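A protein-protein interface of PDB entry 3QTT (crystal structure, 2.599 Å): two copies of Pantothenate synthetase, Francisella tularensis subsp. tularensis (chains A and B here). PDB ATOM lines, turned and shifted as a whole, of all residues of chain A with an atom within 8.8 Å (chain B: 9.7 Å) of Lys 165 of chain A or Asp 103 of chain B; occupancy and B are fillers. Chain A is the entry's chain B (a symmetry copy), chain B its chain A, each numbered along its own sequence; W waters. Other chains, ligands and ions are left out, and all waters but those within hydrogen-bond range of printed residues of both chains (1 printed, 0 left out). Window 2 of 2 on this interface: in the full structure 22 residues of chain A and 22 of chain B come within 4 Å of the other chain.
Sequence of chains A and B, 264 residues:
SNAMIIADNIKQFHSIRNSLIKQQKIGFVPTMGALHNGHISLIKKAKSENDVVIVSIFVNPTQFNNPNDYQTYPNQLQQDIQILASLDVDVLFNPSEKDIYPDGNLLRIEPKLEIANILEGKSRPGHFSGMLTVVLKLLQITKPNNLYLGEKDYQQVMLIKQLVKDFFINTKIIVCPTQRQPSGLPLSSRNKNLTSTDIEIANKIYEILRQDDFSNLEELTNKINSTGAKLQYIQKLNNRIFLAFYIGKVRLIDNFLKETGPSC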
ATOM      1  N   LYS A 112      22.660   8.977 -19.596  1.00  0.00           N
ATOM      2  CA  LYS A 112      23.080   7.751 -18.914  1.00  0.00           C
ATOM      3  C   LYS A 112      24.445   7.963 -18.326  1.00  0.00           C
ATOM      4  O   LYS A 112      25.441   7.837 -19.006  1.00  0.00           O
ATOM      5  CB  LYS A 112      23.142   6.564 -19.873  1.00  0.00           C
ATOM      6  CG  LYS A 112      21.791   5.921 -20.161  1.00  0.00           C
ATOM      7  CD  LYS A 112      20.894   6.863 -20.952  1.00  0.00           C
ATOM      8  CE  LYS A 112      19.519   6.277 -21.191  1.00  0.00           C
ATOM      9  NZ  LYS A 112      18.866   7.009 -22.311  1.00  0.00           N
ATOM     10  N   LEU A 113      24.475   8.196 -17.031  1.00  0.00           N
ATOM     11  CA  LEU A 113      25.690   8.320 -16.264  1.00  0.00           C
ATOM     12  C   LEU A 113      25.209   8.122 -14.836  1.00  0.00           C
ATOM     13  O   LEU A 113      24.023   8.305 -14.557  1.00  0.00           O
ATOM     14  CB  LEU A 113      26.349   9.697 -16.400  1.00  0.00           C
ATOM     15  CG  LEU A 113      26.002  10.828 -17.371  1.00  0.00           C
ATOM     16  CD1 LEU A 113      24.530  11.178 -17.352  1.00  0.00           C
ATOM     17  CD2 LEU A 113      26.847  12.063 -17.019  1.00  0.00           C
ATOM     18  N   LEU A 139      19.897  27.379 -24.810  1.00  0.00           N
ATOM     19  CA  LEU A 139      21.230  27.752 -25.265  1.00  0.00           C
ATOM     20  C   LEU A 139      21.298  27.897 -26.777  1.00  0.00           C
ATOM     21  O   LEU A 139      21.875  28.862 -27.296  1.00  0.00           O
ATOM     22  CB  LEU A 139      22.266  26.750 -24.800  1.00  0.00           C
ATOM     23  CG  LEU A 139      22.683  26.883 -23.345  1.00  0.00           C
ATOM     24  CD1 LEU A 139      23.503  25.679 -22.950  1.00  0.00           C
ATOM     25  CD2 LEU A 139      23.478  28.159 -23.147  1.00  0.00           C
ATOM     26  N   MET A 158      26.771  19.908 -13.138  1.00  0.00           N
ATOM     27  CA  MET A 158      27.664  18.921 -13.701  1.00  0.00           C
ATOM     28  C   MET A 158      27.093  18.498 -15.045  1.00  0.00           C
ATOM     29  O   MET A 158      27.803  18.397 -16.048  1.00  0.00           O
ATOM     30  CB  MET A 158      27.786  17.725 -12.755  1.00  0.00           C
ATOM     31  CG  MET A 158      28.642  17.986 -11.509  1.00  0.00           C
ATOM     32  SD  MET A 158      28.839  16.411 -10.352  1.00  0.00           S
ATOM     33  CE  MET A 158      30.064  15.367 -11.457  1.00  0.00           C
ATOM     34  N   LEU A 159      25.785  18.281 -15.054  1.00  0.00           N
ATOM     35  CA  LEU A 159      25.109  17.783 -16.221  1.00  0.00           C
ATOM     36  C   LEU A 159      25.158  18.765 -17.400  1.00  0.00           C
ATOM     37  O   LEU A 159      25.242  18.364 -18.559  1.00  0.00           O
ATOM     38  CB  LEU A 159      23.678  17.419 -15.860  1.00  0.00           C
ATOM     39  CG  LEU A 159      23.563  16.086 -15.104  1.00  0.00           C
ATOM     40  CD1 LEU A 159      22.119  15.725 -14.818  1.00  0.00           C
ATOM     41  CD2 LEU A 159      24.245  14.963 -15.848  1.00  0.00           C
ATOM     42  N   ILE A 160      25.110  20.049 -17.088  1.00  0.00           N
ATOM     43  CA  ILE A 160      25.059  21.071 -18.103  1.00  0.00           C
ATOM     44  C   ILE A 160      26.450  21.223 -18.628  1.00  0.00           C
ATOM     45  O   ILE A 160      26.633  21.542 -19.790  1.00  0.00           O
ATOM     46  CB  ILE A 160      24.533  22.415 -17.541  1.00  0.00           C
ATOM     47  CG1 ILE A 160      23.045  22.324 -17.231  1.00  0.00           C
ATOM     48  CG2 ILE A 160      24.710  23.528 -18.537  1.00  0.00           C
ATOM     49  CD1 ILE A 160      22.513  23.570 -16.580  1.00  0.00           C
ATOM     50  N   LYS A 161      27.441  20.962 -17.784  1.00  0.00           N
ATOM     51  CA  LYS A 161      28.830  20.964 -18.240  1.00  0.00           C
ATOM     52  C   LYS A 161      29.078  19.853 -19.248  1.00  0.00           C
ATOM     53  O   LYS A 161      29.775  20.028 -20.256  1.00  0.00           O
ATOM     54  CB  LYS A 161      29.793  20.840 -17.068  1.00  0.00           C
ATOM     55  CG  LYS A 161      30.023  22.137 -16.268  1.00  0.00           C
ATOM     56  CD  LYS A 161      30.727  21.803 -14.967  1.00  0.00           C
ATOM     57  CE  LYS A 161      31.336  23.008 -14.283  1.00  0.00           C
ATOM     58  NZ  LYS A 161      32.073  22.538 -13.046  1.00  0.00           N
ATOM     59  N   GLN A 162      28.490  18.701 -18.990  1.00  0.00           N
ATOM     60  CA  GLN A 162      28.579  17.626 -19.949  1.00  0.00           C
ATOM     61  C   GLN A 162      27.886  18.040 -21.241  1.00  0.00           C
ATOM     62  O   GLN A 162      28.505  18.049 -22.314  1.00  0.00           O
ATOM     63  CB  GLN A 162      27.940  16.371 -19.399  1.00  0.00           C
ATOM     64  CG  GLN A 162      28.258  15.140 -20.218  1.00  0.00           C
ATOM     65  CD  GLN A 162      29.733  14.831 -20.219  1.00  0.00           C
ATOM     66  OE1 GLN A 162      30.451  15.122 -19.251  1.00  0.00           O
ATOM     67  NE2 GLN A 162      30.208  14.248 -21.319  1.00  0.00           N
ATOM     68  N   LEU A 163      26.619  18.449 -21.109  1.00  0.00           N
ATOM     69  CA  LEU A 163      25.764  18.837 -22.239  1.00  0.00           C
ATOM     70  C   LEU A 163      26.474  19.772 -23.204  1.00  0.00           C
ATOM     71  O   LEU A 163      26.462  19.554 -24.405  1.00  0.00           O
ATOM     72  CB  LEU A 163      24.526  19.558 -21.732  1.00  0.00           C
ATOM     73  CG  LEU A 163      23.569  20.085 -22.801  1.00  0.00           C
ATOM     74  CD1 LEU A 163      22.746  18.935 -23.392  1.00  0.00           C
ATOM     75  CD2 LEU A 163      22.634  21.142 -22.239  1.00  0.00           C
ATOM     76  N   VAL A 164      27.118  20.793 -22.657  1.00  0.00           N
ATOM     77  CA  VAL A 164      27.818  21.797 -23.452  1.00  0.00           C
ATOM     78  C   VAL A 164      28.995  21.219 -24.237  1.00  0.00           C
ATOM     79  O   VAL A 164      29.245  21.606 -25.389  1.00  0.00           O
ATOM     80  CB  VAL A 164      28.312  22.922 -22.556  1.00  0.00           C
ATOM     81  CG1 VAL A 164      29.462  23.609 -23.182  1.00  0.00           C
ATOM     82  CG2 VAL A 164      27.169  23.935 -22.219  1.00  0.00           C
ATOM     83  N   LYS A 165      29.709  20.297 -23.609  1.00  0.00           N
ATOM     84  CA  LYS A 165      30.882  19.712 -24.198  1.00  0.00           C
ATOM     85  C   LYS A 165      30.469  18.669 -25.262  1.00  0.00           C
ATOM     86  O   LYS A 165      31.078  18.573 -26.348  1.00  0.00           O
ATOM     87  CB  LYS A 165      31.698  19.054 -23.101  1.00  0.00           C
ATOM     88  CG  LYS A 165      32.868  18.226 -23.596  1.00  0.00           C
ATOM     89  CD  LYS A 165      33.330  17.241 -22.548  1.00  0.00           C
ATOM     90  CE  LYS A 165      34.652  16.630 -22.955  1.00  0.00           C
ATOM     91  NZ  LYS A 165      35.296  15.883 -21.844  1.00  0.00           N
ATOM     92  N   ASP A 166      29.433  17.895 -24.941  1.00  0.00           N
ATOM     93  CA  ASP A 166      28.928  16.857 -25.841  1.00  0.00           C
ATOM     94  C   ASP A 166      28.303  17.429 -27.137  1.00  0.00           C
ATOM     95  O   ASP A 166      28.416  16.851 -28.209  1.00  0.00           O
ATOM     96  CB  ASP A 166      27.941  15.952 -25.096  1.00  0.00           C
ATOM     97  CG  ASP A 166      28.538  14.592 -24.776  1.00  0.00           C
ATOM     98  OD1 ASP A 166      29.187  14.025 -25.676  1.00  0.00           O
ATOM     99  OD2 ASP A 166      28.374  14.082 -23.643  1.00  0.00           O
ATOM    100  N   PHE A 167      27.615  18.548 -27.004  1.00  0.00           N
ATOM    101  CA  PHE A 167      26.957  19.240 -28.105  1.00  0.00           C
ATOM    102  C   PHE A 167      27.672  20.398 -28.759  1.00  0.00           C
ATOM    103  O   PHE A 167      27.050  21.188 -29.473  1.00  0.00           O
ATOM    104  CB  PHE A 167      25.479  19.431 -27.822  1.00  0.00           C
ATOM    105  CG  PHE A 167      24.795  18.122 -27.623  1.00  0.00           C
ATOM    106  CD1 PHE A 167      24.688  17.228 -28.680  1.00  0.00           C
ATOM    107  CD2 PHE A 167      24.375  17.728 -26.380  1.00  0.00           C
ATOM    108  CE1 PHE A 167      24.102  15.999 -28.502  1.00  0.00           C
ATOM    109  CE2 PHE A 167      23.796  16.512 -26.187  1.00  0.00           C
ATOM    110  CZ  PHE A 167      23.657  15.640 -27.256  1.00  0.00           C
ATOM    111  N   PHE A 168      28.940  20.569 -28.387  1.00  0.00           N
ATOM    112  CA  PHE A 168      29.857  21.503 -29.049  1.00  0.00           C
ATOM    113  C   PHE A 168      29.323  22.921 -29.127  1.00  0.00           C
ATOM    114  O   PHE A 168      29.348  23.554 -30.185  1.00  0.00           O
ATOM    115  CB  PHE A 168      30.254  21.000 -30.442  1.00  0.00           C
ATOM    116  CG  PHE A 168      30.751  19.584 -30.443  1.00  0.00           C
ATOM    117  CD1 PHE A 168      32.077  19.303 -30.157  1.00  0.00           C
ATOM    118  CD2 PHE A 168      29.892  18.534 -30.714  1.00  0.00           C
ATOM    119  CE1 PHE A 168      32.526  18.010 -30.120  1.00  0.00           C
ATOM    120  CE2 PHE A 168      30.332  17.232 -30.689  1.00  0.00           C
ATOM    121  CZ  PHE A 168      31.655  16.960 -30.389  1.00  0.00           C
ATOM    122  N   ILE A 169      28.843  23.406 -27.993  1.00  0.00           N
ATOM    123  CA  ILE A 169      28.365  24.770 -27.863  1.00  0.00           C
ATOM    124  C   ILE A 169      29.467  25.598 -27.231  1.00  0.00           C
ATOM    125  O   ILE A 169      29.952  25.236 -26.151  1.00  0.00           O
ATOM    126  CB  ILE A 169      27.245  24.777 -26.843  1.00  0.00           C
ATOM    127  CG1 ILE A 169      26.324  23.599 -27.083  1.00  0.00           C
ATOM    128  CG2 ILE A 169      26.482  26.062 -26.881  1.00  0.00           C
ATOM    129  CD1 ILE A 169      25.205  23.547 -26.103  1.00  0.00           C
ATOM    130  N   ASN A 170      29.884  26.703 -27.844  1.00  0.00           N
ATOM    131  CA  ASN A 170      30.950  27.439 -27.177  1.00  0.00           C
ATOM    132  C   ASN A 170      30.346  28.494 -26.253  1.00  0.00           C
ATOM    133  O   ASN A 170      29.945  29.585 -26.677  1.00  0.00           O
ATOM    134  CB  ASN A 170      31.930  28.060 -28.192  1.00  0.00           C
ATOM    135  CG  ASN A 170      33.382  28.099 -27.676  1.00  0.00           C
ATOM    136  OD1 ASN A 170      34.209  28.876 -28.166  1.00  0.00           O
ATOM    137  ND2 ASN A 170      33.687  27.261 -26.682  1.00  0.00           N
ATOM    138  N   THR A 171      30.347  28.153 -24.967  1.00  0.00           N
ATOM    139  CA  THR A 171      29.873  29.024 -23.916  1.00  0.00           C
ATOM    140  C   THR A 171      30.661  28.603 -22.738  1.00  0.00           C
ATOM    141  O   THR A 171      30.814  27.408 -22.506  1.00  0.00           O
ATOM    142  CB  THR A 171      28.425  28.739 -23.532  1.00  0.00           C
ATOM    143  OG1 THR A 171      27.792  28.001 -24.573  1.00  0.00           O
ATOM    144  CG2 THR A 171      27.650  30.032 -23.267  1.00  0.00           C
ATOM    145  N   ILE A 173      30.943  27.995 -18.833  1.00  0.00           N
ATOM    146  CA  ILE A 173      30.098  27.880 -17.685  1.00  0.00           C
ATOM    147  C   ILE A 173      30.777  28.537 -16.474  1.00  0.00           C
ATOM    148  O   ILE A 173      31.957  28.276 -16.176  1.00  0.00           O
ATOM    149  CB  ILE A 173      29.687  26.461 -17.454  1.00  0.00           C
ATOM    150  CG1 ILE A 173      28.721  26.074 -18.556  1.00  0.00           C
ATOM    151  CG2 ILE A 173      28.946  26.334 -16.139  1.00  0.00           C
ATOM    152  CD1 ILE A 173      27.974  24.782 -18.268  1.00  0.00           C
ATOM    153  N   ILE B  10      38.457  16.631 -34.945  1.00  0.00           N
ATOM    154  CA  ILE B  10      37.742  17.866 -34.695  1.00  0.00           C
ATOM    155  C   ILE B  10      38.591  19.141 -34.712  1.00  0.00           C
ATOM    156  O   ILE B  10      38.216  20.135 -35.328  1.00  0.00           O
ATOM    157  CB  ILE B  10      37.006  17.786 -33.363  1.00  0.00           C
ATOM    158  CG1 ILE B  10      35.873  16.769 -33.462  1.00  0.00           C
ATOM    159  CG2 ILE B  10      36.430  19.148 -32.983  1.00  0.00           C
ATOM    160  CD1 ILE B  10      34.589  17.247 -32.837  1.00  0.00           C
ATOM    161  N   HIS B  14      37.572  22.139 -36.871  1.00  0.00           N
ATOM    162  CA  HIS B  14      37.267  23.444 -36.295  1.00  0.00           C
ATOM    163  C   HIS B  14      38.037  24.586 -36.921  1.00  0.00           C
ATOM    164  O   HIS B  14      37.489  25.666 -37.146  1.00  0.00           O
ATOM    165  CB  HIS B  14      37.561  23.454 -34.791  1.00  0.00           C
ATOM    166  CG  HIS B  14      36.462  22.888 -33.970  1.00  0.00           C
ATOM    167  ND1 HIS B  14      35.136  23.005 -34.331  1.00  0.00           N
ATOM    168  CD2 HIS B  14      36.478  22.178 -32.819  1.00  0.00           C
ATOM    169  CE1 HIS B  14      34.384  22.397 -33.435  1.00  0.00           C
ATOM    170  NE2 HIS B  14      35.174  21.888 -32.505  1.00  0.00           N
ATOM    171  N   THR B  62      26.672   3.953 -32.242  1.00  0.00           N
ATOM    172  CA  THR B  62      25.511   3.953 -31.348  1.00  0.00           C
ATOM    173  C   THR B  62      24.194   3.753 -32.088  1.00  0.00           C
ATOM    174  O   THR B  62      23.134   3.587 -31.468  1.00  0.00           O
ATOM    175  CB  THR B  62      25.422   5.228 -30.436  1.00  0.00           C
ATOM    176  OG1 THR B  62      24.929   6.356 -31.183  1.00  0.00           O
ATOM    177  CG2 THR B  62      26.774   5.557 -29.805  1.00  0.00           C
ATOM    178  N   GLU B  97      35.604   7.661 -33.172  1.00  0.00           N
ATOM    179  CA  GLU B  97      34.550   7.568 -32.174  1.00  0.00           C
ATOM    180  C   GLU B  97      34.947   8.463 -31.010  1.00  0.00           C
ATOM    181  O   GLU B  97      34.150   9.249 -30.515  1.00  0.00           O
ATOM    182  CB  GLU B  97      34.368   6.105 -31.758  1.00  0.00           C
ATOM    183  CG  GLU B  97      33.468   5.868 -30.568  1.00  0.00           C
ATOM    184  CD  GLU B  97      33.330   4.379 -30.208  1.00  0.00           C
ATOM    185  OE1 GLU B  97      33.962   3.521 -30.878  1.00  0.00           O
ATOM    186  OE2 GLU B  97      32.566   4.069 -29.261  1.00  0.00           O
ATOM    187  N   LYS B  98      36.211   8.364 -30.617  1.00  0.00           N
ATOM    188  CA  LYS B  98      36.775   9.185 -29.562  1.00  0.00           C
ATOM    189  C   LYS B  98      36.567  10.700 -29.734  1.00  0.00           C
ATOM    190  O   LYS B  98      36.406  11.404 -28.729  1.00  0.00           O
ATOM    191  CB  LYS B  98      38.258   8.860 -29.405  1.00  0.00           C
ATOM    192  CG  LYS B  98      38.904   9.482 -28.191  1.00  0.00           C
ATOM    193  CD  LYS B  98      38.238   8.998 -26.912  1.00  0.00           C
ATOM    194  CE  LYS B  98      38.891   9.610 -25.687  1.00  0.00           C
ATOM    195  NZ  LYS B  98      38.196   9.134 -24.483  1.00  0.00           N
ATOM    196  N   ASP B  99      36.588  11.222 -30.965  1.00  0.00           N
ATOM    197  CA  ASP B  99      36.286  12.649 -31.154  1.00  0.00           C
ATOM    198  C   ASP B  99      34.794  12.984 -31.139  1.00  0.00           C
ATOM    199  O   ASP B  99      34.408  14.114 -30.859  1.00  0.00           O
ATOM    200  CB  ASP B  99      36.969  13.364 -32.346  1.00  0.00           C
ATOM    201  CG  ASP B  99      37.940  12.507 -33.124  1.00  0.00           C
ATOM    202  OD1 ASP B  99      37.758  11.284 -33.217  1.00  0.00           O
ATOM    203  OD2 ASP B  99      38.881  13.096 -33.697  1.00  0.00           O
ATOM    204  N   ILE B 100      33.946  12.038 -31.490  1.00  0.00           N
ATOM    205  CA  ILE B 100      32.518  12.320 -31.443  1.00  0.00           C
ATOM    206  C   ILE B 100      31.946  12.139 -30.035  1.00  0.00           C
ATOM    207  O   ILE B 100      30.994  12.798 -29.642  1.00  0.00           O
ATOM    208  CB  ILE B 100      31.733  11.491 -32.469  1.00  0.00           C
ATOM    209  CG1 ILE B 100      32.266  11.738 -33.885  1.00  0.00           C
ATOM    210  CG2 ILE B 100      30.324  11.879 -32.427  1.00  0.00           C
ATOM    211  CD1 ILE B 100      32.305  13.163 -34.290  1.00  0.00           C
ATOM    212  N   TYR B 101      32.542  11.215 -29.295  1.00  0.00           N
ATOM    213  CA  TYR B 101      32.050  10.786 -28.003  1.00  0.00           C
ATOM    214  C   TYR B 101      33.190  10.701 -27.008  1.00  0.00           C
ATOM    215  O   TYR B 101      33.471   9.623 -26.508  1.00  0.00           O
ATOM    216  CB  TYR B 101      31.454   9.384 -28.107  1.00  0.00           C
ATOM    217  CG  TYR B 101      30.255   9.254 -29.005  1.00  0.00           C
ATOM    218  CD1 TYR B 101      28.970   9.581 -28.542  1.00  0.00           C
ATOM    219  CD2 TYR B 101      30.393   8.767 -30.305  1.00  0.00           C
ATOM    220  CE1 TYR B 101      27.873   9.431 -29.353  1.00  0.00           C
ATOM    221  CE2 TYR B 101      29.308   8.626 -31.133  1.00  0.00           C
ATOM    222  CZ  TYR B 101      28.051   8.957 -30.663  1.00  0.00           C
ATOM    223  OH  TYR B 101      26.975   8.816 -31.507  1.00  0.00           O
ATOM    224  N   PRO B 102      33.838  11.830 -26.712  1.00  0.00           N
ATOM    225  CA  PRO B 102      34.996  11.857 -25.798  1.00  0.00           C
ATOM    226  C   PRO B 102      34.736  11.108 -24.481  1.00  0.00           C
ATOM    227  O   PRO B 102      35.626  10.490 -23.914  1.00  0.00           O
ATOM    228  CB  PRO B 102      35.200  13.352 -25.520  1.00  0.00           C
ATOM    229  CG  PRO B 102      33.895  14.023 -25.969  1.00  0.00           C
ATOM    230  CD  PRO B 102      33.387  13.177 -27.095  1.00  0.00           C
ATOM    231  N   ASP B 103      33.525  11.238 -23.976  1.00  0.00           N
ATOM    232  CA  ASP B 103      33.081  10.555 -22.771  1.00  0.00           C
ATOM    233  C   ASP B 103      32.237   9.292 -22.943  1.00  0.00           C
ATOM    234  O   ASP B 103      31.685   8.783 -21.981  1.00  0.00           O
ATOM    235  CB  ASP B 103      32.458  11.558 -21.798  1.00  0.00           C
ATOM    236  CG  ASP B 103      33.401  12.717 -21.494  1.00  0.00           C
ATOM    237  OD1 ASP B 103      34.619  12.498 -21.483  1.00  0.00           O
ATOM    238  OD2 ASP B 103      32.937  13.852 -21.290  1.00  0.00           O
ATOM    239  N   GLY B 104      32.054   8.827 -24.167  1.00  0.00           N
ATOM    240  CA  GLY B 104      31.184   7.685 -24.379  1.00  0.00           C
ATOM    241  C   GLY B 104      29.821   8.274 -24.646  1.00  0.00           C
ATOM    242  O   GLY B 104      29.711   9.488 -24.762  1.00  0.00           O
ATOM    243  N   ASN B 105      28.774   7.468 -24.731  1.00  0.00           N
ATOM    244  CA  ASN B 105      27.532   8.093 -25.065  1.00  0.00           C
ATOM    245  C   ASN B 105      26.739   8.260 -23.766  1.00  0.00           C
ATOM    246  O   ASN B 105      25.953   7.391 -23.403  1.00  0.00           O
ATOM    247  CB  ASN B 105      26.827   7.070 -25.954  1.00  0.00           C
ATOM    248  CG  ASN B 105      25.658   7.635 -26.677  1.00  0.00           C
ATOM    249  OD1 ASN B 105      25.551   8.844 -26.877  1.00  0.00           O
ATOM    250  ND2 ASN B 105      24.765   6.762 -27.087  1.00  0.00           N
ATOM    251  N   LEU B 106      26.858   9.442 -23.150  1.00  0.00           N
ATOM    252  CA  LEU B 106      26.161   9.753 -21.901  1.00  0.00           C
ATOM    253  C   LEU B 106      24.930  10.604 -22.011  1.00  0.00           C
ATOM    254  O   LEU B 106      24.118  10.642 -21.094  1.00  0.00           O
ATOM    255  CB  LEU B 106      27.118  10.442 -20.968  1.00  0.00           C
ATOM    256  CG  LEU B 106      28.509   9.805 -21.002  1.00  0.00           C
ATOM    257  CD1 LEU B 106      29.378  10.445 -19.945  1.00  0.00           C
ATOM    258  CD2 LEU B 106      28.448   8.269 -20.824  1.00  0.00           C
ATOM    259  N   LEU B 107      24.774  11.249 -23.163  1.00  0.00           N
ATOM    260  CA  LEU B 107      23.661  12.143 -23.389  1.00  0.00           C
ATOM    261  C   LEU B 107      23.126  11.816 -24.774  1.00  0.00           C
ATOM    262  O   LEU B 107      23.862  11.851 -25.758  1.00  0.00           O
ATOM    263  CB  LEU B 107      24.098  13.606 -23.283  1.00  0.00           C
ATOM    264  CG  LEU B 107      24.549  14.174 -21.919  1.00  0.00           C
ATOM    265  CD1 LEU B 107      24.992  15.636 -22.028  1.00  0.00           C
ATOM    266  CD2 LEU B 107      23.518  13.993 -20.766  1.00  0.00           C
ATOM    267  N   ARG B 108      21.851  11.454 -24.845  1.00  0.00           N
ATOM    268  CA  ARG B 108      21.307  10.900 -26.066  1.00  0.00           C
ATOM    269  C   ARG B 108      19.987  11.550 -26.341  1.00  0.00           C
ATOM    270  O   ARG B 108      19.276  11.929 -25.406  1.00  0.00           O
ATOM    271  CB  ARG B 108      21.069   9.410 -25.914  1.00  0.00           C
ATOM    272  CG  ARG B 108      22.129   8.709 -25.128  1.00  0.00           C
ATOM    273  CD  ARG B 108      21.660   7.339 -24.781  1.00  0.00           C
ATOM    274  NE  ARG B 108      22.689   6.605 -24.062  1.00  0.00           N
ATOM    275  CZ  ARG B 108      22.842   5.284 -24.112  1.00  0.00           C
ATOM    276  NH1 ARG B 108      22.035   4.543 -24.876  1.00  0.00           N
ATOM    277  NH2 ARG B 108      23.814   4.704 -23.406  1.00  0.00           N
ATOM    278  N   LYS B 137      25.155  16.097 -33.167  1.00  0.00           N
ATOM    279  CA  LYS B 137      26.569  16.446 -32.967  1.00  0.00           C
ATOM    280  C   LYS B 137      27.225  16.883 -34.265  1.00  0.00           C
ATOM    281  O   LYS B 137      28.004  17.832 -34.282  1.00  0.00           O
ATOM    282  CB  LYS B 137      27.381  15.292 -32.357  1.00  0.00           C
ATOM    283  CG  LYS B 137      27.251  15.081 -30.848  1.00  0.00           C
ATOM    284  CD  LYS B 137      27.834  13.731 -30.459  1.00  0.00           C
ATOM    285  CE  LYS B 137      27.735  13.462 -28.973  1.00  0.00           C
ATOM    286  NZ  LYS B 137      28.866  14.067 -28.193  1.00  0.00           N
ATOM    287  N   GLN B 140      26.098  20.437 -35.136  1.00  0.00           N
ATOM    288  CA  GLN B 140      26.688  21.392 -34.230  1.00  0.00           C
ATOM    289  C   GLN B 140      28.113  21.691 -34.637  1.00  0.00           C
ATOM    290  O   GLN B 140      28.554  22.824 -34.587  1.00  0.00           O
ATOM    291  CB  GLN B 140      26.658  20.826 -32.814  1.00  0.00           C
ATOM    292  CG  GLN B 140      25.274  20.796 -32.224  1.00  0.00           C
ATOM    293  CD  GLN B 140      24.728  22.196 -32.041  1.00  0.00           C
ATOM    294  OE1 GLN B 140      24.191  22.785 -32.973  1.00  0.00           O
ATOM    295  NE2 GLN B 140      24.886  22.747 -30.837  1.00  0.00           N
ATOM    296  N   ILE B 141      28.832  20.664 -35.050  1.00  0.00           N
ATOM    297  CA  ILE B 141      30.210  20.823 -35.478  1.00  0.00           C
ATOM    298  C   ILE B 141      30.345  21.524 -36.840  1.00  0.00           C
ATOM    299  O   ILE B 141      31.178  22.420 -37.002  1.00  0.00           O
ATOM    300  CB  ILE B 141      30.881  19.451 -35.597  1.00  0.00           C
ATOM    301  CG1 ILE B 141      31.042  18.773 -34.229  1.00  0.00           C
ATOM    302  CG2 ILE B 141      32.202  19.564 -36.312  1.00  0.00           C
ATOM    303  CD1 ILE B 141      31.144  17.239 -34.389  1.00  0.00           C
HETATM  304  O   HOH W   1      31.172  12.106 -25.094  1.00  0.00           O
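Among the printed residues, pairs that only touch across the chains: Lys 112 of chain A with Arg 108 of chain B, Leu 113 of chain A with Leu 106 of chain B, Gln 162 of chain A with Leu 107 of chain B, Leu 163 of chain A with Leu 107 of chain B, Phe 167 of chain A with Lys 137 of chain B, Phe 168 of chain A with Ile 10 of chain B, Phe 168 of chain A with Asp 99 of chain B, Phe 168 of chain A with Lys 137 of chain B and Phe 168 of chain A with Ile 141 of chain B.
Lys 165 of chain A touches just one residue of chain B: Asp 103 (3.2 Å). Asp 103 of chain B touches two residues of chain A. No residue of chain A comes within 4 Å of Pro 102 of chain B. No residue of chain A comes within 4 Å of Gly 104 of chain B. Printed residues of chain A within 4 Å of Asp 99 of chain B: Phe 168. Of the printed residues of chain A, Arg 108 of chain B touches Lys 112 (3.6 Å). Ile 160 of chain A touches none of the printed residues of chain B. The nearest residue of chain B that does not touch Lys 165 of chain A is Pro 102 of chain B (4.1 Å).
Water W1 lies within hydrogen-bond range of N of Asp 103 of chain B (2.7 Å), OD1 of Asp 166 of chain A (2.8 Å) and O of Gly 104 of chain B (3.0 Å).
OD2 of Asp 103 of chain B is in hydrogen-bond range of NE2 of Gln 162 of chain A (2.8 Å). The side-chain carboxylate (OD2) of Asp 103 of chain B is in salt-bridge range of the side-chain amino group (NZ) of Lys 165 of chain A, 3.2 Å away. The backbone carbonyl oxygen of Leu 106 of chain B lies within hydrogen-bond range of the backbone NH of Lys 112 of chain A (2.7 Å). NZ of Lys 137 of chain B is in salt-bridge range of OD1 of Asp 166 of chain A (2.5 Å). The side-chain amide nitrogen (NE2) of Gln 140 of chain B lies within hydrogen-bond range of the backbone carbonyl oxygen (O) of Phe 167 of chain A.
The backbone carbonyl oxygen of Ile 100 of chain B lies within hydrogen-bond range of the side-chain amino group of Lys 137 of chain B (2.9 Å). O of Asn 105 of chain B is in hydrogen-bond range of NE of Arg 108 of chain B, 3.4 Å away. The side-chain carboxylate (OD2) of Asp 166 of chain A sits at hydrogen-bond distance from the side-chain amide nitrogen (NE2) of Gln 162 of chain A (3.0 Å).
Of the 18 printed residues of chain B, 9 touch a printed residue of chain A. Of the 18 printed residues of chain A, 8 touch a printed residue of chain B. Hydrophobic or aromatic side chains of chain A within 4 Å of the printed part of chain B: Leu 113, Leu 163, Phe 167 and Phe 168. Among the printed residues, 14 pairs touch across the chains.
No position is printed for both chains. Of the 14 pairs that touch across the chains among the printed residues, none has its exchanged pair printed and touching as well.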
